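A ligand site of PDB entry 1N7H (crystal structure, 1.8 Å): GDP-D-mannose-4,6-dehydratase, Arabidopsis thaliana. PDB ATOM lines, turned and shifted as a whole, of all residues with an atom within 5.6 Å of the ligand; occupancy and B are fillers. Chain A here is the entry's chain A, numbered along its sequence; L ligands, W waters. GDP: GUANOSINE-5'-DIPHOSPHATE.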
ATOM      1  N   SER A 117      11.782 -14.253 -21.790  1.00  0.00           N
ATOM      2  CA  SER A 117      11.652 -15.295 -20.768  1.00  0.00           C
ATOM      3  C   SER A 117      12.357 -16.633 -20.920  1.00  0.00           C
ATOM      4  O   SER A 117      12.172 -17.513 -20.070  1.00  0.00           O
ATOM      5  CB  SER A 117      10.168 -15.583 -20.527  1.00  0.00           C
ATOM      6  OG  SER A 117       9.621 -16.318 -21.611  1.00  0.00           O
ATOM      7  N   HIS A 118      13.161 -16.800 -21.960  1.00  0.00           N
ATOM      8  CA  HIS A 118      13.813 -18.083 -22.164  1.00  0.00           C
ATOM      9  C   HIS A 118      15.227 -18.074 -21.615  1.00  0.00           C
ATOM     10  O   HIS A 118      16.032 -17.206 -21.937  1.00  0.00           O
ATOM     11  CB  HIS A 118      13.794 -18.458 -23.647  1.00  0.00           C
ATOM     12  CG  HIS A 118      13.977 -19.918 -23.896  1.00  0.00           C
ATOM     13  ND1 HIS A 118      15.189 -20.553 -23.753  1.00  0.00           N
ATOM     14  CD2 HIS A 118      13.075 -20.897 -24.187  1.00  0.00           C
ATOM     15  CE1 HIS A 118      15.039 -21.851 -23.951  1.00  0.00           C
ATOM     16  NE2 HIS A 118      13.761 -22.088 -24.204  1.00  0.00           N
ATOM     17  N   VAL A 119      15.516 -19.068 -20.774  1.00  0.00           N
ATOM     18  CA  VAL A 119      16.826 -19.194 -20.151  1.00  0.00           C
ATOM     19  C   VAL A 119      17.953 -19.463 -21.131  1.00  0.00           C
ATOM     20  O   VAL A 119      18.992 -18.796 -21.070  1.00  0.00           O
ATOM     21  CB  VAL A 119      16.805 -20.311 -19.070  1.00  0.00           C
ATOM     22  CG1 VAL A 119      18.212 -20.580 -18.559  1.00  0.00           C
ATOM     23  CG2 VAL A 119      15.912 -19.878 -17.904  1.00  0.00           C
ATOM     24  N   GLU A 164      13.570 -19.446 -11.132  1.00  0.00           N
ATOM     25  CA  GLU A 164      14.880 -19.480 -11.753  1.00  0.00           C
ATOM     26  C   GLU A 164      15.864 -18.656 -10.896  1.00  0.00           C
ATOM     27  O   GLU A 164      17.078 -18.857 -10.932  1.00  0.00           O
ATOM     28  CB  GLU A 164      14.771 -18.893 -13.167  1.00  0.00           C
ATOM     29  CG  GLU A 164      15.744 -19.451 -14.185  1.00  0.00           C
ATOM     30  CD  GLU A 164      15.649 -20.961 -14.355  1.00  0.00           C
ATOM     31  OE1 GLU A 164      14.572 -21.564 -14.129  1.00  0.00           O
ATOM     32  OE2 GLU A 164      16.671 -21.557 -14.742  1.00  0.00           O
ATOM     33  N   ASN A 214       7.915 -22.944 -12.496  1.00  0.00           N
ATOM     34  CA  ASN A 214       7.501 -23.250 -13.852  1.00  0.00           C
ATOM     35  C   ASN A 214       6.005 -23.533 -14.017  1.00  0.00           C
ATOM     36  O   ASN A 214       5.442 -24.347 -13.294  1.00  0.00           O
ATOM     37  CB  ASN A 214       8.266 -24.470 -14.386  1.00  0.00           C
ATOM     38  CG  ASN A 214       9.769 -24.229 -14.469  1.00  0.00           C
ATOM     39  OD1 ASN A 214      10.408 -23.922 -13.475  1.00  0.00           O
ATOM     40  ND2 ASN A 214      10.327 -24.400 -15.667  1.00  0.00           N
ATOM     41  N   GLU A 216       3.095 -24.235 -17.197  1.00  0.00           N
ATOM     42  CA  GLU A 216       2.889 -24.527 -18.592  1.00  0.00           C
ATOM     43  C   GLU A 216       1.408 -24.544 -18.951  1.00  0.00           C
ATOM     44  O   GLU A 216       0.543 -24.328 -18.102  1.00  0.00           O
ATOM     45  CB  GLU A 216       3.503 -25.892 -18.898  1.00  0.00           C
ATOM     46  CG  GLU A 216       4.671 -26.270 -17.966  1.00  0.00           C
ATOM     47  CD  GLU A 216       5.927 -25.431 -18.193  1.00  0.00           C
ATOM     48  OE1 GLU A 216       6.351 -24.719 -17.255  1.00  0.00           O
ATOM     49  OE2 GLU A 216       6.488 -25.486 -19.300  1.00  0.00           O
ATOM     50  N   ARG A 220       1.907 -22.555 -23.945  1.00  0.00           N
ATOM     51  CA  ARG A 220       3.323 -22.410 -23.600  1.00  0.00           C
ATOM     52  C   ARG A 220       4.168 -22.282 -24.871  1.00  0.00           C
ATOM     53  O   ARG A 220       3.860 -22.915 -25.889  1.00  0.00           O
ATOM     54  CB  ARG A 220       3.763 -23.639 -22.798  1.00  0.00           C
ATOM     55  CG  ARG A 220       5.225 -23.678 -22.377  1.00  0.00           C
ATOM     56  CD  ARG A 220       5.574 -22.530 -21.460  1.00  0.00           C
ATOM     57  NE  ARG A 220       6.492 -22.933 -20.400  1.00  0.00           N
ATOM     58  CZ  ARG A 220       7.339 -22.102 -19.784  1.00  0.00           C
ATOM     59  NH1 ARG A 220       7.391 -20.824 -20.136  1.00  0.00           N
ATOM     60  NH2 ARG A 220       8.088 -22.539 -18.789  1.00  0.00           N
ATOM     61  N   ASN A 223       9.443 -23.460 -27.488  1.00  0.00           N
ATOM     62  CA  ASN A 223      10.869 -23.604 -27.212  1.00  0.00           C
ATOM     63  C   ASN A 223      11.135 -24.058 -25.785  1.00  0.00           C
ATOM     64  O   ASN A 223      12.278 -24.344 -25.428  1.00  0.00           O
ATOM     65  CB  ASN A 223      11.610 -22.280 -27.506  1.00  0.00           C
ATOM     66  CG  ASN A 223      13.109 -22.458 -27.620  1.00  0.00           C
ATOM     67  OD1 ASN A 223      13.591 -23.458 -28.159  1.00  0.00           O
ATOM     68  ND2 ASN A 223      13.865 -21.468 -27.142  1.00  0.00           N
ATOM     69  N   PHE A 224      10.091 -24.109 -24.950  1.00  0.00           N
ATOM     70  CA  PHE A 224      10.246 -24.593 -23.578  1.00  0.00           C
ATOM     71  C   PHE A 224      10.103 -26.107 -23.630  1.00  0.00           C
ATOM     72  O   PHE A 224       9.375 -26.640 -24.479  1.00  0.00           O
ATOM     73  CB  PHE A 224       9.244 -23.921 -22.641  1.00  0.00           C
ATOM     74  CG  PHE A 224       9.479 -22.433 -22.495  1.00  0.00           C
ATOM     75  CD1 PHE A 224       8.879 -21.527 -23.359  1.00  0.00           C
ATOM     76  CD2 PHE A 224      10.390 -21.965 -21.554  1.00  0.00           C
ATOM     77  CE1 PHE A 224       9.161 -20.160 -23.274  1.00  0.00           C
ATOM     78  CE2 PHE A 224      10.685 -20.602 -21.465  1.00  0.00           C
ATOM     79  CZ  PHE A 224      10.079 -19.697 -22.337  1.00  0.00           C
ATOM     80  N   VAL A 225      10.783 -26.816 -22.733  1.00  0.00           N
ATOM     81  CA  VAL A 225      10.800 -28.278 -22.815  1.00  0.00           C
ATOM     82  C   VAL A 225       9.471 -29.030 -22.804  1.00  0.00           C
ATOM     83  O   VAL A 225       9.290 -29.977 -23.562  1.00  0.00           O
ATOM     84  CB  VAL A 225      11.770 -28.879 -21.728  1.00  0.00           C
ATOM     85  CG1 VAL A 225      11.101 -28.977 -20.371  1.00  0.00           C
ATOM     86  CG2 VAL A 225      12.281 -30.232 -22.212  1.00  0.00           C
ATOM     87  N   THR A 226       8.519 -28.597 -21.975  1.00  0.00           N
ATOM     88  CA  THR A 226       7.241 -29.285 -21.891  1.00  0.00           C
ATOM     89  C   THR A 226       6.484 -29.211 -23.217  1.00  0.00           C
ATOM     90  O   THR A 226       6.063 -30.236 -23.755  1.00  0.00           O
ATOM     91  CB  THR A 226       6.379 -28.681 -20.785  1.00  0.00           C
ATOM     92  OG1 THR A 226       6.202 -27.281 -21.033  1.00  0.00           O
ATOM     93  CG2 THR A 226       7.052 -28.870 -19.426  1.00  0.00           C
ATOM     94  N   LYS A 228       7.704 -28.330 -26.105  1.00  0.00           N
ATOM     95  CA  LYS A 228       8.516 -28.912 -27.160  1.00  0.00           C
ATOM     96  C   LYS A 228       8.208 -30.406 -27.234  1.00  0.00           C
ATOM     97  O   LYS A 228       8.062 -30.973 -28.323  1.00  0.00           O
ATOM     98  CB  LYS A 228      10.008 -28.700 -26.854  1.00  0.00           C
ATOM     99  CG  LYS A 228      10.934 -29.377 -27.862  1.00  0.00           C
ATOM    100  CD  LYS A 228      12.397 -29.093 -27.580  1.00  0.00           C
ATOM    101  CE  LYS A 228      13.299 -29.772 -28.609  1.00  0.00           C
ATOM    102  NZ  LYS A 228      14.741 -29.379 -28.436  1.00  0.00           N
ATOM    103  N   PHE A 245      14.649 -34.311 -30.435  1.00  0.00           N
ATOM    104  CA  PHE A 245      15.967 -34.028 -29.891  1.00  0.00           C
ATOM    105  C   PHE A 245      15.878 -33.175 -28.635  1.00  0.00           C
ATOM    106  O   PHE A 245      15.284 -32.096 -28.649  1.00  0.00           O
ATOM    107  CB  PHE A 245      16.824 -33.331 -30.942  1.00  0.00           C
ATOM    108  CG  PHE A 245      17.030 -34.153 -32.183  1.00  0.00           C
ATOM    109  CD1 PHE A 245      16.087 -34.159 -33.201  1.00  0.00           C
ATOM    110  CD2 PHE A 245      18.152 -34.961 -32.317  1.00  0.00           C
ATOM    111  CE1 PHE A 245      16.259 -34.959 -34.329  1.00  0.00           C
ATOM    112  CE2 PHE A 245      18.338 -35.763 -33.440  1.00  0.00           C
ATOM    113  CZ  PHE A 245      17.379 -35.759 -34.451  1.00  0.00           C
ATOM    114  N   LEU A 246      16.482 -33.679 -27.557  1.00  0.00           N
ATOM    115  CA  LEU A 246      16.472 -32.977 -26.279  1.00  0.00           C
ATOM    116  C   LEU A 246      17.855 -32.916 -25.650  1.00  0.00           C
ATOM    117  O   LEU A 246      18.820 -33.461 -26.195  1.00  0.00           O
ATOM    118  CB  LEU A 246      15.500 -33.686 -25.320  1.00  0.00           C
ATOM    119  CG  LEU A 246      14.035 -33.655 -25.737  1.00  0.00           C
ATOM    120  CD1 LEU A 246      13.237 -34.668 -24.913  1.00  0.00           C
ATOM    121  CD2 LEU A 246      13.486 -32.242 -25.545  1.00  0.00           C
ATOM    122  N   GLY A 247      17.944 -32.232 -24.517  1.00  0.00           N
ATOM    123  CA  GLY A 247      19.212 -32.102 -23.819  1.00  0.00           C
ATOM    124  C   GLY A 247      19.272 -32.903 -22.540  1.00  0.00           C
ATOM    125  O   GLY A 247      19.293 -34.139 -22.570  1.00  0.00           O
ATOM    126  N   ASN A 248      19.282 -32.200 -21.409  1.00  0.00           N
ATOM    127  CA  ASN A 248      19.371 -32.811 -20.084  1.00  0.00           C
ATOM    128  C   ASN A 248      18.029 -33.327 -19.589  1.00  0.00           C
ATOM    129  O   ASN A 248      17.150 -32.552 -19.203  1.00  0.00           O
ATOM    130  CB  ASN A 248      19.945 -31.781 -19.101  1.00  0.00           C
ATOM    131  CG  ASN A 248      19.985 -32.286 -17.674  1.00  0.00           C
ATOM    132  OD1 ASN A 248      20.019 -33.487 -17.431  1.00  0.00           O
ATOM    133  ND2 ASN A 248      19.992 -31.359 -16.716  1.00  0.00           N
ATOM    134  N   LEU A 249      17.866 -34.653 -19.590  1.00  0.00           N
ATOM    135  CA  LEU A 249      16.610 -35.262 -19.164  1.00  0.00           C
ATOM    136  C   LEU A 249      16.496 -35.412 -17.652  1.00  0.00           C
ATOM    137  O   LEU A 249      15.427 -35.758 -17.142  1.00  0.00           O
ATOM    138  CB  LEU A 249      16.425 -36.631 -19.818  1.00  0.00           C
ATOM    139  CG  LEU A 249      16.528 -36.708 -21.341  1.00  0.00           C
ATOM    140  CD1 LEU A 249      16.195 -38.118 -21.794  1.00  0.00           C
ATOM    141  CD2 LEU A 249      15.595 -35.686 -21.984  1.00  0.00           C
ATOM    142  N   ALA A 251      17.053 -32.969 -15.376  1.00  0.00           N
ATOM    143  CA  ALA A 251      16.688 -31.740 -14.689  1.00  0.00           C
ATOM    144  C   ALA A 251      15.314 -31.958 -14.076  1.00  0.00           C
ATOM    145  O   ALA A 251      14.439 -32.532 -14.723  1.00  0.00           O
ATOM    146  CB  ALA A 251      16.636 -30.570 -15.675  1.00  0.00           C
ATOM    147  N   ARG A 253      11.855 -30.284 -12.250  1.00  0.00           N
ATOM    148  CA  ARG A 253      11.085 -29.064 -12.101  1.00  0.00           C
ATOM    149  C   ARG A 253       9.739 -29.278 -11.434  1.00  0.00           C
ATOM    150  O   ARG A 253       9.186 -30.380 -11.422  1.00  0.00           O
ATOM    151  CB  ARG A 253      10.844 -28.429 -13.479  1.00  0.00           C
ATOM    152  CG  ARG A 253      12.110 -27.967 -14.191  1.00  0.00           C
ATOM    153  CD  ARG A 253      12.623 -26.650 -13.589  1.00  0.00           C
ATOM    154  NE  ARG A 253      13.803 -26.148 -14.292  1.00  0.00           N
ATOM    155  CZ  ARG A 253      15.037 -26.627 -14.128  1.00  0.00           C
ATOM    156  NH1 ARG A 253      16.046 -26.106 -14.811  1.00  0.00           N
ATOM    157  NH2 ARG A 253      15.261 -27.627 -13.280  1.00  0.00           N
ATOM    158  N   TRP A 255       6.197 -28.238 -11.969  1.00  0.00           N
ATOM    159  CA  TRP A 255       5.383 -27.758 -13.077  1.00  0.00           C
ATOM    160  C   TRP A 255       3.889 -27.630 -12.750  1.00  0.00           C
ATOM    161  O   TRP A 255       3.259 -28.626 -12.375  1.00  0.00           O
ATOM    162  CB  TRP A 255       5.510 -28.694 -14.277  1.00  0.00           C
ATOM    163  CG  TRP A 255       6.796 -28.585 -15.061  1.00  0.00           C
ATOM    164  CD1 TRP A 255       7.252 -27.485 -15.750  1.00  0.00           C
ATOM    165  CD2 TRP A 255       7.716 -29.642 -15.333  1.00  0.00           C
ATOM    166  NE1 TRP A 255       8.410 -27.809 -16.433  1.00  0.00           N
ATOM    167  CE2 TRP A 255       8.707 -29.126 -16.209  1.00  0.00           C
ATOM    168  CE3 TRP A 255       7.794 -30.987 -14.938  1.00  0.00           C
ATOM    169  CZ2 TRP A 255       9.768 -29.912 -16.684  1.00  0.00           C
ATOM    170  CZ3 TRP A 255       8.851 -31.760 -15.414  1.00  0.00           C
ATOM    171  CH2 TRP A 255       9.827 -31.219 -16.274  1.00  0.00           C
ATOM    172  N   VAL A 287      12.515 -34.242 -16.474  1.00  0.00           N
ATOM    173  CA  VAL A 287      12.099 -34.148 -17.865  1.00  0.00           C
ATOM    174  C   VAL A 287      11.838 -35.595 -18.331  1.00  0.00           C
ATOM    175  O   VAL A 287      10.942 -35.853 -19.125  1.00  0.00           O
ATOM    176  CB  VAL A 287      13.217 -33.501 -18.732  1.00  0.00           C
ATOM    177  CG1 VAL A 287      12.877 -33.602 -20.210  1.00  0.00           C
ATOM    178  CG2 VAL A 287      13.398 -32.031 -18.330  1.00  0.00           C
ATOM    179  N   TYR A 312      21.547 -28.636 -26.744  1.00  0.00           N
ATOM    180  CA  TYR A 312      20.448 -28.184 -25.899  1.00  0.00           C
ATOM    181  C   TYR A 312      20.825 -28.086 -24.420  1.00  0.00           C
ATOM    182  O   TYR A 312      20.002 -27.716 -23.586  1.00  0.00           O
ATOM    183  CB  TYR A 312      19.218 -29.074 -26.087  1.00  0.00           C
ATOM    184  CG  TYR A 312      18.641 -28.935 -27.470  1.00  0.00           C
ATOM    185  CD1 TYR A 312      18.659 -30.001 -28.375  1.00  0.00           C
ATOM    186  CD2 TYR A 312      18.140 -27.707 -27.918  1.00  0.00           C
ATOM    187  CE1 TYR A 312      18.204 -29.850 -29.682  1.00  0.00           C
ATOM    188  CE2 TYR A 312      17.681 -27.543 -29.226  1.00  0.00           C
ATOM    189  CZ  TYR A 312      17.719 -28.616 -30.106  1.00  0.00           C
ATOM    190  OH  TYR A 312      17.287 -28.442 -31.396  1.00  0.00           O
ATOM    191  N   PHE A 313      22.076 -28.421 -24.096  1.00  0.00           N
ATOM    192  CA  PHE A 313      22.550 -28.317 -22.717  1.00  0.00           C
ATOM    193  C   PHE A 313      22.799 -26.822 -22.473  1.00  0.00           C
ATOM    194  O   PHE A 313      23.113 -26.090 -23.418  1.00  0.00           O
ATOM    195  CB  PHE A 313      23.881 -29.061 -22.503  1.00  0.00           C
ATOM    196  CG  PHE A 313      23.819 -30.559 -22.673  1.00  0.00           C
ATOM    197  CD1 PHE A 313      22.660 -31.269 -22.393  1.00  0.00           C
ATOM    198  CD2 PHE A 313      24.956 -31.266 -23.070  1.00  0.00           C
ATOM    199  CE1 PHE A 313      22.626 -32.667 -22.507  1.00  0.00           C
ATOM    200  CE2 PHE A 313      24.942 -32.651 -23.187  1.00  0.00           C
ATOM    201  CZ  PHE A 313      23.775 -33.356 -22.904  1.00  0.00           C
ATOM    202  N   ARG A 314      22.654 -26.359 -21.234  1.00  0.00           N
ATOM    203  CA  ARG A 314      22.925 -24.952 -20.934  1.00  0.00           C
ATOM    204  C   ARG A 314      24.323 -24.842 -20.339  1.00  0.00           C
ATOM    205  O   ARG A 314      24.815 -25.793 -19.722  1.00  0.00           O
ATOM    206  CB  ARG A 314      21.909 -24.371 -19.930  1.00  0.00           C
ATOM    207  CG  ARG A 314      20.546 -23.956 -20.517  1.00  0.00           C
ATOM    208  CD  ARG A 314      19.652 -25.158 -20.627  1.00  0.00           C
ATOM    209  NE  ARG A 314      18.416 -24.899 -21.353  1.00  0.00           N
ATOM    210  CZ  ARG A 314      17.309 -24.386 -20.820  1.00  0.00           C
ATOM    211  NH1 ARG A 314      16.239 -24.223 -21.580  1.00  0.00           N
ATOM    212  NH2 ARG A 314      17.282 -24.025 -19.547  1.00  0.00           N
ATOM    213  N   GLU A 317      23.624 -25.233 -15.638  1.00  0.00           N
ATOM    214  CA  GLU A 317      22.297 -25.814 -15.428  1.00  0.00           C
ATOM    215  C   GLU A 317      21.703 -25.581 -14.040  1.00  0.00           C
ATOM    216  O   GLU A 317      22.411 -25.333 -13.063  1.00  0.00           O
ATOM    217  CB  GLU A 317      22.368 -27.318 -15.716  1.00  0.00           C
ATOM    218  CG  GLU A 317      21.062 -28.109 -15.577  1.00  0.00           C
ATOM    219  CD  GLU A 317      20.021 -27.723 -16.604  1.00  0.00           C
ATOM    220  OE1 GLU A 317      19.397 -26.656 -16.451  1.00  0.00           O
ATOM    221  OE2 GLU A 317      19.837 -28.500 -17.570  1.00  0.00           O
ATOM    222  N   VAL A 318      20.367 -25.642 -13.985  1.00  0.00           N
ATOM    223  CA  VAL A 318      19.613 -25.525 -12.747  1.00  0.00           C
ATOM    224  C   VAL A 318      19.068 -26.940 -12.592  1.00  0.00           C
ATOM    225  O   VAL A 318      18.186 -27.355 -13.333  1.00  0.00           O
ATOM    226  CB  VAL A 318      18.463 -24.505 -12.876  1.00  0.00           C
ATOM    227  CG1 VAL A 318      17.565 -24.562 -11.650  1.00  0.00           C
ATOM    228  CG2 VAL A 318      19.060 -23.103 -13.013  1.00  0.00           C
ATOM    229  N   LEU A 321      14.282 -27.749  -8.961  1.00  0.00           N
ATOM    230  CA  LEU A 321      13.426 -26.722  -8.385  1.00  0.00           C
ATOM    231  C   LEU A 321      12.155 -27.363  -7.869  1.00  0.00           C
ATOM    232  O   LEU A 321      11.500 -28.127  -8.575  1.00  0.00           O
ATOM    233  CB  LEU A 321      13.072 -25.666  -9.441  1.00  0.00           C
ATOM    234  CG  LEU A 321      14.221 -24.852 -10.043  1.00  0.00           C
ATOM    235  CD1 LEU A 321      13.677 -23.934 -11.126  1.00  0.00           C
ATOM    236  CD2 LEU A 321      14.913 -24.019  -8.978  1.00  0.00           C
HETATM  237  PB  GDP L   1      13.466 -23.279 -17.537  1.00  0.00           P
HETATM  238  O1B GDP L   1      12.875 -21.872 -17.559  1.00  0.00           O
HETATM  239  O2B GDP L   1      14.844 -23.462 -18.165  1.00  0.00           O
HETATM  240  O3B GDP L   1      13.161 -24.133 -16.303  1.00  0.00           O
HETATM  241  O3A GDP L   1      12.535 -23.969 -18.677  1.00  0.00           O
HETATM  242  PA  GDP L   1      12.781 -24.929 -19.971  1.00  0.00           P
HETATM  243  O1A GDP L   1      11.490 -25.610 -20.242  1.00  0.00           O
HETATM  244  O2A GDP L   1      13.446 -24.183 -21.057  1.00  0.00           O
HETATM  245  O5' GDP L   1      13.823 -26.048 -19.506  1.00  0.00           O
HETATM  246  C5' GDP L   1      13.517 -26.891 -18.395  1.00  0.00           C
HETATM  247  C4' GDP L   1      14.635 -27.874 -18.169  1.00  0.00           C
HETATM  248  O4' GDP L   1      14.611 -28.855 -19.249  1.00  0.00           O
HETATM  249  C3' GDP L   1      16.043 -27.275 -18.157  1.00  0.00           C
HETATM  250  O3' GDP L   1      16.845 -27.934 -17.180  1.00  0.00           O
HETATM  251  C2' GDP L   1      16.558 -27.600 -19.557  1.00  0.00           C
HETATM  252  O2' GDP L   1      17.974 -27.729 -19.593  1.00  0.00           O
HETATM  253  C1' GDP L   1      15.912 -28.957 -19.799  1.00  0.00           C
HETATM  254  N9  GDP L   1      15.796 -29.397 -21.180  1.00  0.00           N
HETATM  255  C8  GDP L   1      16.219 -30.608 -21.691  1.00  0.00           C
HETATM  256  N7  GDP L   1      16.136 -30.686 -22.986  1.00  0.00           N
HETATM  257  C5  GDP L   1      15.637 -29.447 -23.365  1.00  0.00           C
HETATM  258  C6  GDP L   1      15.328 -28.944 -24.656  1.00  0.00           C
HETATM  259  O6  GDP L   1      15.464 -29.501 -25.758  1.00  0.00           O
HETATM  260  N1  GDP L   1      14.812 -27.644 -24.592  1.00  0.00           N
HETATM  261  C2  GDP L   1      14.624 -26.930 -23.434  1.00  0.00           C
HETATM  262  N2  GDP L   1      14.095 -25.708 -23.584  1.00  0.00           N
HETATM  263  N3  GDP L   1      14.936 -27.383 -22.229  1.00  0.00           N
HETATM  264  C4  GDP L   1      15.425 -28.639 -22.275  1.00  0.00           C
HETATM  265  O   HOH W   1       9.264 -25.787 -18.334  1.00  0.00           O
HETATM  266  O   HOH W   2      19.275 -29.244 -21.497  1.00  0.00           O
HETATM  267  O   HOH W   3      16.601 -23.573 -16.100  1.00  0.00           O
HETATM  268  O   HOH W   4      14.395 -25.859 -26.812  1.00  0.00           O
HETATM  269  O   HOH W   5      13.766 -21.401 -20.369  1.00  0.00           O
HETATM  270  O   HOH W   6      10.081 -20.869 -17.799  1.00  0.00           O
HETATM  271  O   HOH W   7      12.594 -19.284 -17.724  1.00  0.00           O
HETATM  272  O   HOH W   8      17.852 -25.729 -24.024  1.00  0.00           O
HETATM  273  O   HOH W   9      11.247 -21.040 -15.548  1.00  0.00           O
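O6 of the ligand sits at hydrogen-bond distance from NZ of Lys 228 (2.8 Å). The backbone NH of Gly 247 sits at hydrogen-bond distance from a nitrogen (N7) of the ligand (2.8 Å). The guanidinium group (NH1) of Arg 314 lies within salt-bridge range of an oxygen (O2A) of the ligand (2.8 Å). The backbone NH (N) of Val 225 sits at hydrogen-bond distance from an oxygen (O1A) of the ligand (2.9 Å). The side-chain carboxylate (OE2) of Glu 317 sits at hydrogen-bond distance from an oxygen (O2') of the ligand (2.9 Å). The side-chain amide nitrogen (ND2) of Asn 214 is in hydrogen-bond range of an oxygen (O3B) of the ligand. NE of Arg 253 is in salt-bridge range of O3B of the ligand (2.9 Å). N2 of the ligand sits at hydrogen-bond distance from O of Asn 223, at 2.9 Å.
The backbone carbonyl oxygen of Phe 245 lies within hydrogen-bond range of the side-chain amino group of Lys 228. NH1 of Arg 253 lies within salt-bridge range of OE1 of Glu 317, 3.8 Å away. OE2 of Glu 317 sits at hydrogen-bond distance from ND2 of Asn 248. The guanidinium group of Arg 253 lies within hydrogen-bond range of the backbone carbonyl oxygen of Val 318 (2.9 Å). NE2 of His 118 sits at hydrogen-bond distance from O of Asn 223 (3.0 Å). The backbone NH (N) of Val 287 is in hydrogen-bond range of the backbone carbonyl oxygen (O) of Ala 251 (3.1 Å). The backbone NH of Val 287 is in hydrogen-bond range of the backbone carbonyl oxygen of Leu 249, 3.4 Å away.
Residues that only touch the ligand: His 118, Val 119, Glu 164, Phe 224, Phe 245, Leu 246, Asn 248, Ala 251, Val 287 and Tyr 312. Hydrophobic or aromatic side chains within 4 Å of the ligand: His 118, Val 119, Phe 224, Val 225, Leu 246, Ala 251, Val 287 and Tyr 312. The nearest printed residue that does not touch the ligand is Val 318 (4.1 Å).
Water W7 bridges an oxygen (O1B) of the ligand (2.6 Å) and the backbone carbonyl oxygen (O) of Ser 117 (3.0 Å). Water W3 lies within hydrogen-bond range of OE2 of Glu 164 (2.4 Å), O2B of the ligand (2.7 Å) and NH1 of Arg 253 (2.9 Å). Water W9 bridges O1B of the ligand and ND2 of Asn 214. Water W5 lies within hydrogen-bond range of an oxygen (O2A) of the ligand and the backbone NH (N) of Val 119. Water W6 lies within hydrogen-bond range of the guanidinium group of Arg 220 (2.8 Å) and an oxygen (O1B) of the ligand (3.0 Å). Water W8 bridges the guanidinium group (NE) of Arg 314 and the backbone carbonyl oxygen (O) of Tyr 312.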
